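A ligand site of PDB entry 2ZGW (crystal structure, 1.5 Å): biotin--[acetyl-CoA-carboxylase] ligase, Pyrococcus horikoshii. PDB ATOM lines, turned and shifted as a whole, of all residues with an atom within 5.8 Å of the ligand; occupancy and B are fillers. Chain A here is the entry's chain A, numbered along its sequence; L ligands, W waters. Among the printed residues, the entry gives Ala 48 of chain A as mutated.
The backbone carbonyl oxygen of Leu 62 lies within hydrogen-bond range of the backbone NH of Ile 128, at 2.8 Å.
N of Trp 53 lies within hydrogen-bond range of O of Gly 45, at 3.0 Å.
The side-chain amide nitrogen (NE2) of Gln 42 sits at hydrogen-bond distance from the side-chain hydroxyl (OG) of Ser 55.
N of Thr 22 sits at hydrogen-bond distance from OE1 of Gln 42 (2.8 Å).
N of Gly 127 lies within hydrogen-bond range of O of Leu 116, 2.8 Å away.
The side-chain hydroxyl (OG) of Ser 55 lies within hydrogen-bond range of the backbone carbonyl oxygen (O) of Trp 53.
The backbone carbonyl oxygen (O) of Leu 116 lies within hydrogen-bond range of the side-chain amide nitrogen (ND2) of Asn 23.
N of Glu 24 is in hydrogen-bond range of OG of Ser 21 (3.2 Å).
The backbone carbonyl oxygen (O) of Ile 128 lies close to a sulfur (S1) of the ligand, 3.8 Å away.
Asn 23 touches the ligand.
Gly 45 touches the ligand (CA to O3, 3.6 Å).
CA of Gly 47 touches O2 of the ligand, 3.4 Å away.
Trp 53 touches the ligand (CZ3 to O1, 3.6 Å).
Leu 62 touches the ligand.
Ser 63 touches the ligand.
ND2 of Asn 103 touches C1 of the ligand (3.5 Å).
Gly 114 touches the ligand (CA to O1, 3.5 Å).
Val 115 touches the ligand.
CB of Leu 116 touches C4 of the ligand (3.8 Å).
Gly 129 touches the ligand.
Hydrophobic or aromatic side chains that line the ligand: His 46, Ala 48, Trp 53 and Leu 116.
Within 4 Å of the ligand: Ser 21, Thr 22, Asn 23, Gln 42, Gly 45, His 46, Gly 47, Ala 48, Arg 51, Trp 53, Leu 62, Ser 63, Asn 103, Asp 104, Gly 114, Val 115, Leu 116, Ile 128 and Gly 129.
The nearest printed residue that does not touch the ligand is Trp 61 (4.1 Å).
Water W1 lies within hydrogen-bond range of OD1 of Asp 104, NH2 of Arg 51, O2 of the ligand and ND2 of Asn 103.
N of Ala 48 lies within hydrogen-bond range of O2 of the ligand, at 2.7 Å.
N of His 46 sits at hydrogen-bond distance from O3 of the ligand (2.9 Å).
The side-chain amide oxygen (OE1) of Gln 42 lies within hydrogen-bond range of a nitrogen (N1) of the ligand.
The guanidinium group (NH1) of Arg 51 lies within salt-bridge range of an oxygen (O1) of the ligand (2.7 Å).
OG of Ser 21 sits at hydrogen-bond distance from O3 of the ligand.
O of His 46 is in hydrogen-bond range of N2 of the ligand (2.8 Å).
The side-chain hydroxyl (OG1) of Thr 22 is in hydrogen-bond range of a nitrogen (N1) of the ligand (3.1 Å).
An oxygen (O1) of the ligand sits close to the side-chain carboxylate of Asp 104, 3.0 Å away.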
ATOM      1  N   THR A  20      -6.003  24.451 -11.104  1.00  0.00           N
ATOM      2  CA  THR A  20      -6.427  23.357 -11.959  1.00  0.00           C
ATOM      3  C   THR A  20      -5.167  22.790 -12.613  1.00  0.00           C
ATOM      4  O   THR A  20      -4.858  21.611 -12.488  1.00  0.00           O
ATOM      5  CB  THR A  20      -7.389  23.856 -13.052  1.00  0.00           C
ATOM      6  OG1 THR A  20      -6.832  25.027 -13.678  1.00  0.00           O
ATOM      7  CG2 THR A  20      -8.739  24.215 -12.444  1.00  0.00           C
ATOM      8  N   SER A  21      -4.442  23.661 -13.308  1.00  0.00           N
ATOM      9  CA  SER A  21      -3.199  23.285 -13.990  1.00  0.00           C
ATOM     10  C   SER A  21      -2.392  24.535 -14.242  1.00  0.00           C
ATOM     11  O   SER A  21      -2.905  25.525 -14.753  1.00  0.00           O
ATOM     12  CB  SER A  21      -3.528  22.611 -15.336  1.00  0.00           C
ATOM     13  OG  SER A  21      -2.388  22.619 -16.190  1.00  0.00           O
ATOM     14  N   THR A  22      -1.107  24.510 -13.869  1.00  0.00           N
ATOM     15  CA  THR A  22      -0.256  25.673 -14.087  1.00  0.00           C
ATOM     16  C   THR A  22      -0.058  25.922 -15.583  1.00  0.00           C
ATOM     17  O   THR A  22       0.066  27.064 -16.015  1.00  0.00           O
ATOM     18  CB  THR A  22       1.120  25.504 -13.393  1.00  0.00           C
ATOM     19  OG1 THR A  22       1.780  24.332 -13.891  1.00  0.00           O
ATOM     20  CG2 THR A  22       0.961  25.365 -11.883  1.00  0.00           C
ATOM     21  N   ASN A  23      -0.048  24.858 -16.387  1.00  0.00           N
ATOM     22  CA  ASN A  23       0.115  25.022 -17.831  1.00  0.00           C
ATOM     23  C   ASN A  23      -1.099  25.720 -18.420  1.00  0.00           C
ATOM     24  O   ASN A  23      -0.967  26.596 -19.279  1.00  0.00           O
ATOM     25  CB  ASN A  23       0.341  23.665 -18.514  1.00  0.00           C
ATOM     26  CG  ASN A  23       1.789  23.450 -18.932  1.00  0.00           C
ATOM     27  OD1 ASN A  23       2.705  23.820 -18.212  1.00  0.00           O
ATOM     28  ND2 ASN A  23       1.979  22.839 -20.095  1.00  0.00           N
ATOM     29  N   GLU A  24      -2.289  25.321 -17.979  1.00  0.00           N
ATOM     30  CA  GLU A  24      -3.509  25.939 -18.485  1.00  0.00           C
ATOM     31  C   GLU A  24      -3.590  27.411 -18.074  1.00  0.00           C
ATOM     32  O   GLU A  24      -3.942  28.273 -18.882  1.00  0.00           O
ATOM     33  CB  GLU A  24      -4.741  25.201 -17.969  1.00  0.00           C
ATOM     34  CG  GLU A  24      -4.886  23.774 -18.502  1.00  0.00           C
ATOM     35  CD  GLU A  24      -4.851  23.698 -20.013  1.00  0.00           C
ATOM     36  OE1 GLU A  24      -5.627  24.423 -20.673  1.00  0.00           O
ATOM     37  OE2 GLU A  24      -4.045  22.906 -20.556  1.00  0.00           O
ATOM     38  N   GLN A  42      -2.249  20.481  -7.954  1.00  0.00           N
ATOM     39  CA  GLN A  42      -3.063  20.712  -9.142  1.00  0.00           C
ATOM     40  C   GLN A  42      -4.215  19.732  -9.106  1.00  0.00           C
ATOM     41  O   GLN A  42      -4.028  18.554  -8.775  1.00  0.00           O
ATOM     42  CB  GLN A  42      -2.265  20.483 -10.430  1.00  0.00           C
ATOM     43  CG  GLN A  42      -1.026  21.345 -10.572  1.00  0.00           C
ATOM     44  CD  GLN A  42      -0.344  21.159 -11.909  1.00  0.00           C
ATOM     45  OE1 GLN A  42      -0.221  22.103 -12.690  1.00  0.00           O
ATOM     46  NE2 GLN A  42       0.109  19.942 -12.183  1.00  0.00           N
ATOM     47  N   MET A  44      -6.161  19.259 -11.830  1.00  0.00           N
ATOM     48  CA  MET A  44      -6.289  18.755 -13.194  1.00  0.00           C
ATOM     49  C   MET A  44      -4.943  18.752 -13.921  1.00  0.00           C
ATOM     50  O   MET A  44      -4.831  19.252 -15.042  1.00  0.00           O
ATOM     51  CB  MET A  44      -7.293  19.622 -13.969  1.00  0.00           C
ATOM     52  CG  MET A  44      -8.631  19.793 -13.279  1.00  0.00           C
ATOM     53  SD  MET A  44      -9.811  20.736 -14.255  1.00  0.00           S
ATOM     54  CE  MET A  44     -10.759  19.401 -15.004  1.00  0.00           C
ATOM     55  N   GLY A  45      -3.924  18.209 -13.272  1.00  0.00           N
ATOM     56  CA  GLY A  45      -2.608  18.146 -13.882  1.00  0.00           C
ATOM     57  C   GLY A  45      -2.666  17.363 -15.173  1.00  0.00           C
ATOM     58  O   GLY A  45      -3.330  16.317 -15.237  1.00  0.00           O
ATOM     59  N   HIS A  46      -1.976  17.851 -16.205  1.00  0.00           N
ATOM     60  CA  HIS A  46      -1.964  17.207 -17.516  1.00  0.00           C
ATOM     61  C   HIS A  46      -0.574  16.805 -17.967  1.00  0.00           C
ATOM     62  O   HIS A  46       0.407  17.525 -17.739  1.00  0.00           O
ATOM     63  CB  HIS A  46      -2.505  18.162 -18.601  1.00  0.00           C
ATOM     64  CG  HIS A  46      -3.822  18.794 -18.260  1.00  0.00           C
ATOM     65  ND1 HIS A  46      -3.951  20.137 -17.977  1.00  0.00           N
ATOM     66  CD2 HIS A  46      -5.058  18.265 -18.125  1.00  0.00           C
ATOM     67  CE1 HIS A  46      -5.212  20.414 -17.693  1.00  0.00           C
ATOM     68  NE2 HIS A  46      -5.907  19.289 -17.776  1.00  0.00           N
ATOM     69  N   GLY A  47      -0.489  15.661 -18.639  1.00  0.00           N
ATOM     70  CA  GLY A  47       0.787  15.198 -19.154  1.00  0.00           C
ATOM     71  C   GLY A  47       0.674  15.241 -20.664  1.00  0.00           C
ATOM     72  O   GLY A  47      -0.324  15.727 -21.194  1.00  0.00           O
ATOM     73  N   ALA A  48       1.682  14.719 -21.363  1.00  0.00           N
ATOM     74  CA  ALA A  48       1.665  14.709 -22.820  1.00  0.00           C
ATOM     75  C   ALA A  48       0.635  13.712 -23.327  1.00  0.00           C
ATOM     76  O   ALA A  48       0.315  12.725 -22.657  1.00  0.00           O
ATOM     77  CB  ALA A  48       3.045  14.360 -23.353  1.00  0.00           C
ATOM     78  N   ARG A  51      -2.664  12.725 -21.035  1.00  0.00           N
ATOM     79  CA  ARG A  51      -2.580  11.862 -19.861  1.00  0.00           C
ATOM     80  C   ARG A  51      -2.828  12.677 -18.589  1.00  0.00           C
ATOM     81  O   ARG A  51      -2.696  13.899 -18.592  1.00  0.00           O
ATOM     82  CB  ARG A  51      -1.198  11.228 -19.730  1.00  0.00           C
ATOM     83  CG  ARG A  51      -0.107  12.275 -19.546  1.00  0.00           C
ATOM     84  CD  ARG A  51       0.927  11.851 -18.519  1.00  0.00           C
ATOM     85  NE  ARG A  51       1.841  10.839 -19.028  1.00  0.00           N
ATOM     86  CZ  ARG A  51       3.107  10.705 -18.657  1.00  0.00           C
ATOM     87  NH1 ARG A  51       3.635  11.519 -17.761  1.00  0.00           N
ATOM     88  NH2 ARG A  51       3.846   9.749 -19.201  1.00  0.00           N
ATOM     89  N   TRP A  53      -1.712  13.788 -14.867  1.00  0.00           N
ATOM     90  CA  TRP A  53      -0.499  13.886 -14.078  1.00  0.00           C
ATOM     91  C   TRP A  53      -0.883  14.159 -12.624  1.00  0.00           C
ATOM     92  O   TRP A  53      -1.417  15.219 -12.300  1.00  0.00           O
ATOM     93  CB  TRP A  53       0.392  15.007 -14.619  1.00  0.00           C
ATOM     94  CG  TRP A  53       1.675  15.152 -13.872  1.00  0.00           C
ATOM     95  CD1 TRP A  53       1.911  15.988 -12.811  1.00  0.00           C
ATOM     96  CD2 TRP A  53       2.891  14.417 -14.078  1.00  0.00           C
ATOM     97  NE1 TRP A  53       3.200  15.820 -12.355  1.00  0.00           N
ATOM     98  CE2 TRP A  53       3.824  14.870 -13.119  1.00  0.00           C
ATOM     99  CE3 TRP A  53       3.286  13.431 -14.992  1.00  0.00           C
ATOM    100  CZ2 TRP A  53       5.127  14.357 -13.040  1.00  0.00           C
ATOM    101  CZ3 TRP A  53       4.574  12.929 -14.919  1.00  0.00           C
ATOM    102  CH2 TRP A  53       5.484  13.393 -13.944  1.00  0.00           C
ATOM    103  N   SER A  55      -0.732  15.390  -9.107  1.00  0.00           N
ATOM    104  CA  SER A  55      -0.041  16.544  -8.548  1.00  0.00           C
ATOM    105  C   SER A  55      -0.424  16.854  -7.102  1.00  0.00           C
ATOM    106  O   SER A  55      -0.947  17.932  -6.808  1.00  0.00           O
ATOM    107  CB  SER A  55      -0.325  17.775  -9.411  1.00  0.00           C
ATOM    108  OG  SER A  55      -0.156  17.475 -10.795  1.00  0.00           O
ATOM    109  N   LEU A  60       6.759  19.581  -6.909  1.00  0.00           N
ATOM    110  CA  LEU A  60       7.011  20.866  -7.550  1.00  0.00           C
ATOM    111  C   LEU A  60       6.271  20.872  -8.893  1.00  0.00           C
ATOM    112  O   LEU A  60       6.668  20.182  -9.840  1.00  0.00           O
ATOM    113  CB  LEU A  60       8.518  21.077  -7.761  1.00  0.00           C
ATOM    114  CG  LEU A  60       8.958  22.473  -8.214  1.00  0.00           C
ATOM    115  CD1 LEU A  60       8.546  23.502  -7.177  1.00  0.00           C
ATOM    116  CD2 LEU A  60      10.467  22.495  -8.421  1.00  0.00           C
ATOM    117  N   TRP A  61       5.210  21.663  -8.951  1.00  0.00           N
ATOM    118  CA  TRP A  61       4.375  21.760 -10.142  1.00  0.00           C
ATOM    119  C   TRP A  61       4.440  23.201 -10.646  1.00  0.00           C
ATOM    120  O   TRP A  61       3.884  24.106 -10.012  1.00  0.00           O
ATOM    121  CB  TRP A  61       2.919  21.393  -9.797  1.00  0.00           C
ATOM    122  CG  TRP A  61       2.788  20.274  -8.785  1.00  0.00           C
ATOM    123  CD1 TRP A  61       2.123  20.331  -7.585  1.00  0.00           C
ATOM    124  CD2 TRP A  61       3.343  18.954  -8.870  1.00  0.00           C
ATOM    125  NE1 TRP A  61       2.230  19.135  -6.926  1.00  0.00           N
ATOM    126  CE2 TRP A  61       2.975  18.275  -7.695  1.00  0.00           C
ATOM    127  CE3 TRP A  61       4.121  18.296  -9.825  1.00  0.00           C
ATOM    128  CZ2 TRP A  61       3.356  16.945  -7.448  1.00  0.00           C
ATOM    129  CZ3 TRP A  61       4.502  16.966  -9.579  1.00  0.00           C
ATOM    130  CH2 TRP A  61       4.109  16.311  -8.395  1.00  0.00           C
ATOM    131  N   LEU A  62       5.107  23.422 -11.771  1.00  0.00           N
ATOM    132  CA  LEU A  62       5.229  24.777 -12.274  1.00  0.00           C
ATOM    133  C   LEU A  62       5.263  24.886 -13.798  1.00  0.00           C
ATOM    134  O   LEU A  62       5.485  23.904 -14.498  1.00  0.00           O
ATOM    135  CB  LEU A  62       6.489  25.436 -11.691  1.00  0.00           C
ATOM    136  CG  LEU A  62       7.869  24.822 -11.971  1.00  0.00           C
ATOM    137  CD1 LEU A  62       8.342  25.164 -13.377  1.00  0.00           C
ATOM    138  CD2 LEU A  62       8.861  25.363 -10.952  1.00  0.00           C
ATOM    139  N   SER A  63       5.009  26.095 -14.269  1.00  0.00           N
ATOM    140  CA  SER A  63       5.021  26.403 -15.691  1.00  0.00           C
ATOM    141  C   SER A  63       5.732  27.730 -15.852  1.00  0.00           C
ATOM    142  O   SER A  63       5.665  28.589 -14.972  1.00  0.00           O
ATOM    143  CB  SER A  63       3.603  26.503 -16.253  1.00  0.00           C
ATOM    144  OG  SER A  63       2.909  25.284 -16.122  1.00  0.00           O
ATOM    145  N   ASN A 103      10.845  13.923 -23.017  1.00  0.00           N
ATOM    146  CA  ASN A 103      10.400  14.804 -21.943  1.00  0.00           C
ATOM    147  C   ASN A 103      10.368  14.272 -20.512  1.00  0.00           C
ATOM    148  O   ASN A 103       9.930  14.987 -19.613  1.00  0.00           O
ATOM    149  CB  ASN A 103       8.994  15.275 -22.295  1.00  0.00           C
ATOM    150  CG  ASN A 103       7.982  14.141 -22.266  1.00  0.00           C
ATOM    151  OD1 ASN A 103       8.269  13.028 -22.721  1.00  0.00           O
ATOM    152  ND2 ASN A 103       6.801  14.414 -21.731  1.00  0.00           N
ATOM    153  N   ASP A 104      10.824  13.047 -20.291  1.00  0.00           N
ATOM    154  CA  ASP A 104      10.765  12.479 -18.956  1.00  0.00           C
ATOM    155  C   ASP A 104      12.132  12.310 -18.307  1.00  0.00           C
ATOM    156  O   ASP A 104      13.149  12.179 -18.997  1.00  0.00           O
ATOM    157  CB  ASP A 104      10.069  11.108 -18.985  1.00  0.00           C
ATOM    158  CG  ASP A 104       8.691  11.177 -19.607  1.00  0.00           C
ATOM    159  OD1 ASP A 104       7.881  12.016 -19.176  1.00  0.00           O
ATOM    160  OD2 ASP A 104       8.426  10.368 -20.538  1.00  0.00           O
ATOM    161  N   ALA A 113      10.096  12.915 -12.890  1.00  0.00           N
ATOM    162  CA  ALA A 113       9.664  14.190 -13.436  1.00  0.00           C
ATOM    163  C   ALA A 113       9.191  14.076 -14.874  1.00  0.00           C
ATOM    164  O   ALA A 113       9.581  13.162 -15.611  1.00  0.00           O
ATOM    165  CB  ALA A 113      10.801  15.199 -13.343  1.00  0.00           C
ATOM    166  N   GLY A 114       8.351  15.026 -15.269  1.00  0.00           N
ATOM    167  CA  GLY A 114       7.815  15.059 -16.615  1.00  0.00           C
ATOM    168  C   GLY A 114       7.760  16.501 -17.091  1.00  0.00           C
ATOM    169  O   GLY A 114       7.509  17.415 -16.291  1.00  0.00           O
ATOM    170  N   VAL A 115       7.971  16.708 -18.386  1.00  0.00           N
ATOM    171  CA  VAL A 115       7.966  18.036 -18.994  1.00  0.00           C
ATOM    172  C   VAL A 115       6.935  18.120 -20.109  1.00  0.00           C
ATOM    173  O   VAL A 115       6.832  17.214 -20.941  1.00  0.00           O
ATOM    174  CB  VAL A 115       9.362  18.372 -19.572  1.00  0.00           C
ATOM    175  CG1 VAL A 115       9.373  19.790 -20.134  1.00  0.00           C
ATOM    176  CG2 VAL A 115      10.419  18.209 -18.495  1.00  0.00           C
ATOM    177  N   LEU A 116       6.170  19.210 -20.123  1.00  0.00           N
ATOM    178  CA  LEU A 116       5.150  19.422 -21.145  1.00  0.00           C
ATOM    179  C   LEU A 116       5.217  20.846 -21.684  1.00  0.00           C
ATOM    180  O   LEU A 116       4.992  21.809 -20.941  1.00  0.00           O
ATOM    181  CB  LEU A 116       3.753  19.177 -20.577  1.00  0.00           C
ATOM    182  CG  LEU A 116       2.585  19.377 -21.556  1.00  0.00           C
ATOM    183  CD1 LEU A 116       2.677  18.360 -22.680  1.00  0.00           C
ATOM    184  CD2 LEU A 116       1.262  19.241 -20.827  1.00  0.00           C
ATOM    185  N   GLY A 127       6.108  23.529 -19.046  1.00  0.00           N
ATOM    186  CA  GLY A 127       5.597  22.949 -17.815  1.00  0.00           C
ATOM    187  C   GLY A 127       6.480  21.848 -17.289  1.00  0.00           C
ATOM    188  O   GLY A 127       6.958  20.999 -18.054  1.00  0.00           O
ATOM    189  N   ILE A 128       6.696  21.836 -15.980  1.00  0.00           N
ATOM    190  CA  ILE A 128       7.545  20.837 -15.349  1.00  0.00           C
ATOM    191  C   ILE A 128       6.909  20.328 -14.059  1.00  0.00           C
ATOM    192  O   ILE A 128       6.495  21.108 -13.213  1.00  0.00           O
ATOM    193  CB  ILE A 128       8.932  21.412 -14.997  1.00  0.00           C
ATOM    194  CG1 ILE A 128       9.625  21.931 -16.256  1.00  0.00           C
ATOM    195  CG2 ILE A 128       9.793  20.347 -14.311  1.00  0.00           C
ATOM    196  CD1 ILE A 128      10.895  22.725 -15.984  1.00  0.00           C
ATOM    197  N   GLY A 129       6.855  19.003 -13.935  1.00  0.00           N
ATOM    198  CA  GLY A 129       6.320  18.383 -12.742  1.00  0.00           C
ATOM    199  C   GLY A 129       7.412  17.508 -12.160  1.00  0.00           C
ATOM    200  O   GLY A 129       7.916  16.608 -12.843  1.00  0.00           O
HETATM  201  C1  LIG L   1       4.552  14.186 -19.060  1.00  0.00           C
HETATM  202  O1  LIG L   1       5.329  13.453 -18.418  1.00  0.00           O
HETATM  203  O2  LIG L   1       3.788  13.721 -19.961  1.00  0.00           O
HETATM  204  C2  LIG L   1       4.494  15.659 -18.816  1.00  0.00           C
HETATM  205  C3  LIG L   1       4.040  16.034 -17.438  1.00  0.00           C
HETATM  206  C4  LIG L   1       4.060  17.512 -17.193  1.00  0.00           C
HETATM  207  C5  LIG L   1       3.598  17.856 -15.778  1.00  0.00           C
HETATM  208  C6  LIG L   1       3.593  19.337 -15.423  1.00  0.00           C
HETATM  209  S1  LIG L   1       3.048  19.669 -13.761  1.00  0.00           S
HETATM  210  C7  LIG L   1       3.253  21.433 -14.116  1.00  0.00           C
HETATM  211  C8  LIG L   1       2.488  21.550 -15.469  1.00  0.00           C
HETATM  212  N1  LIG L   1       1.025  21.678 -15.300  1.00  0.00           N
HETATM  213  C9  LIG L   1       0.405  20.645 -15.914  1.00  0.00           C
HETATM  214  O3  LIG L   1      -0.835  20.462 -15.950  1.00  0.00           O
HETATM  215  N2  LIG L   1       1.324  19.808 -16.508  1.00  0.00           N
HETATM  216  C10 LIG L   1       2.682  20.271 -16.304  1.00  0.00           C
HETATM  217  O   HOH W   1       5.550  11.503 -20.896  1.00  0.00           O
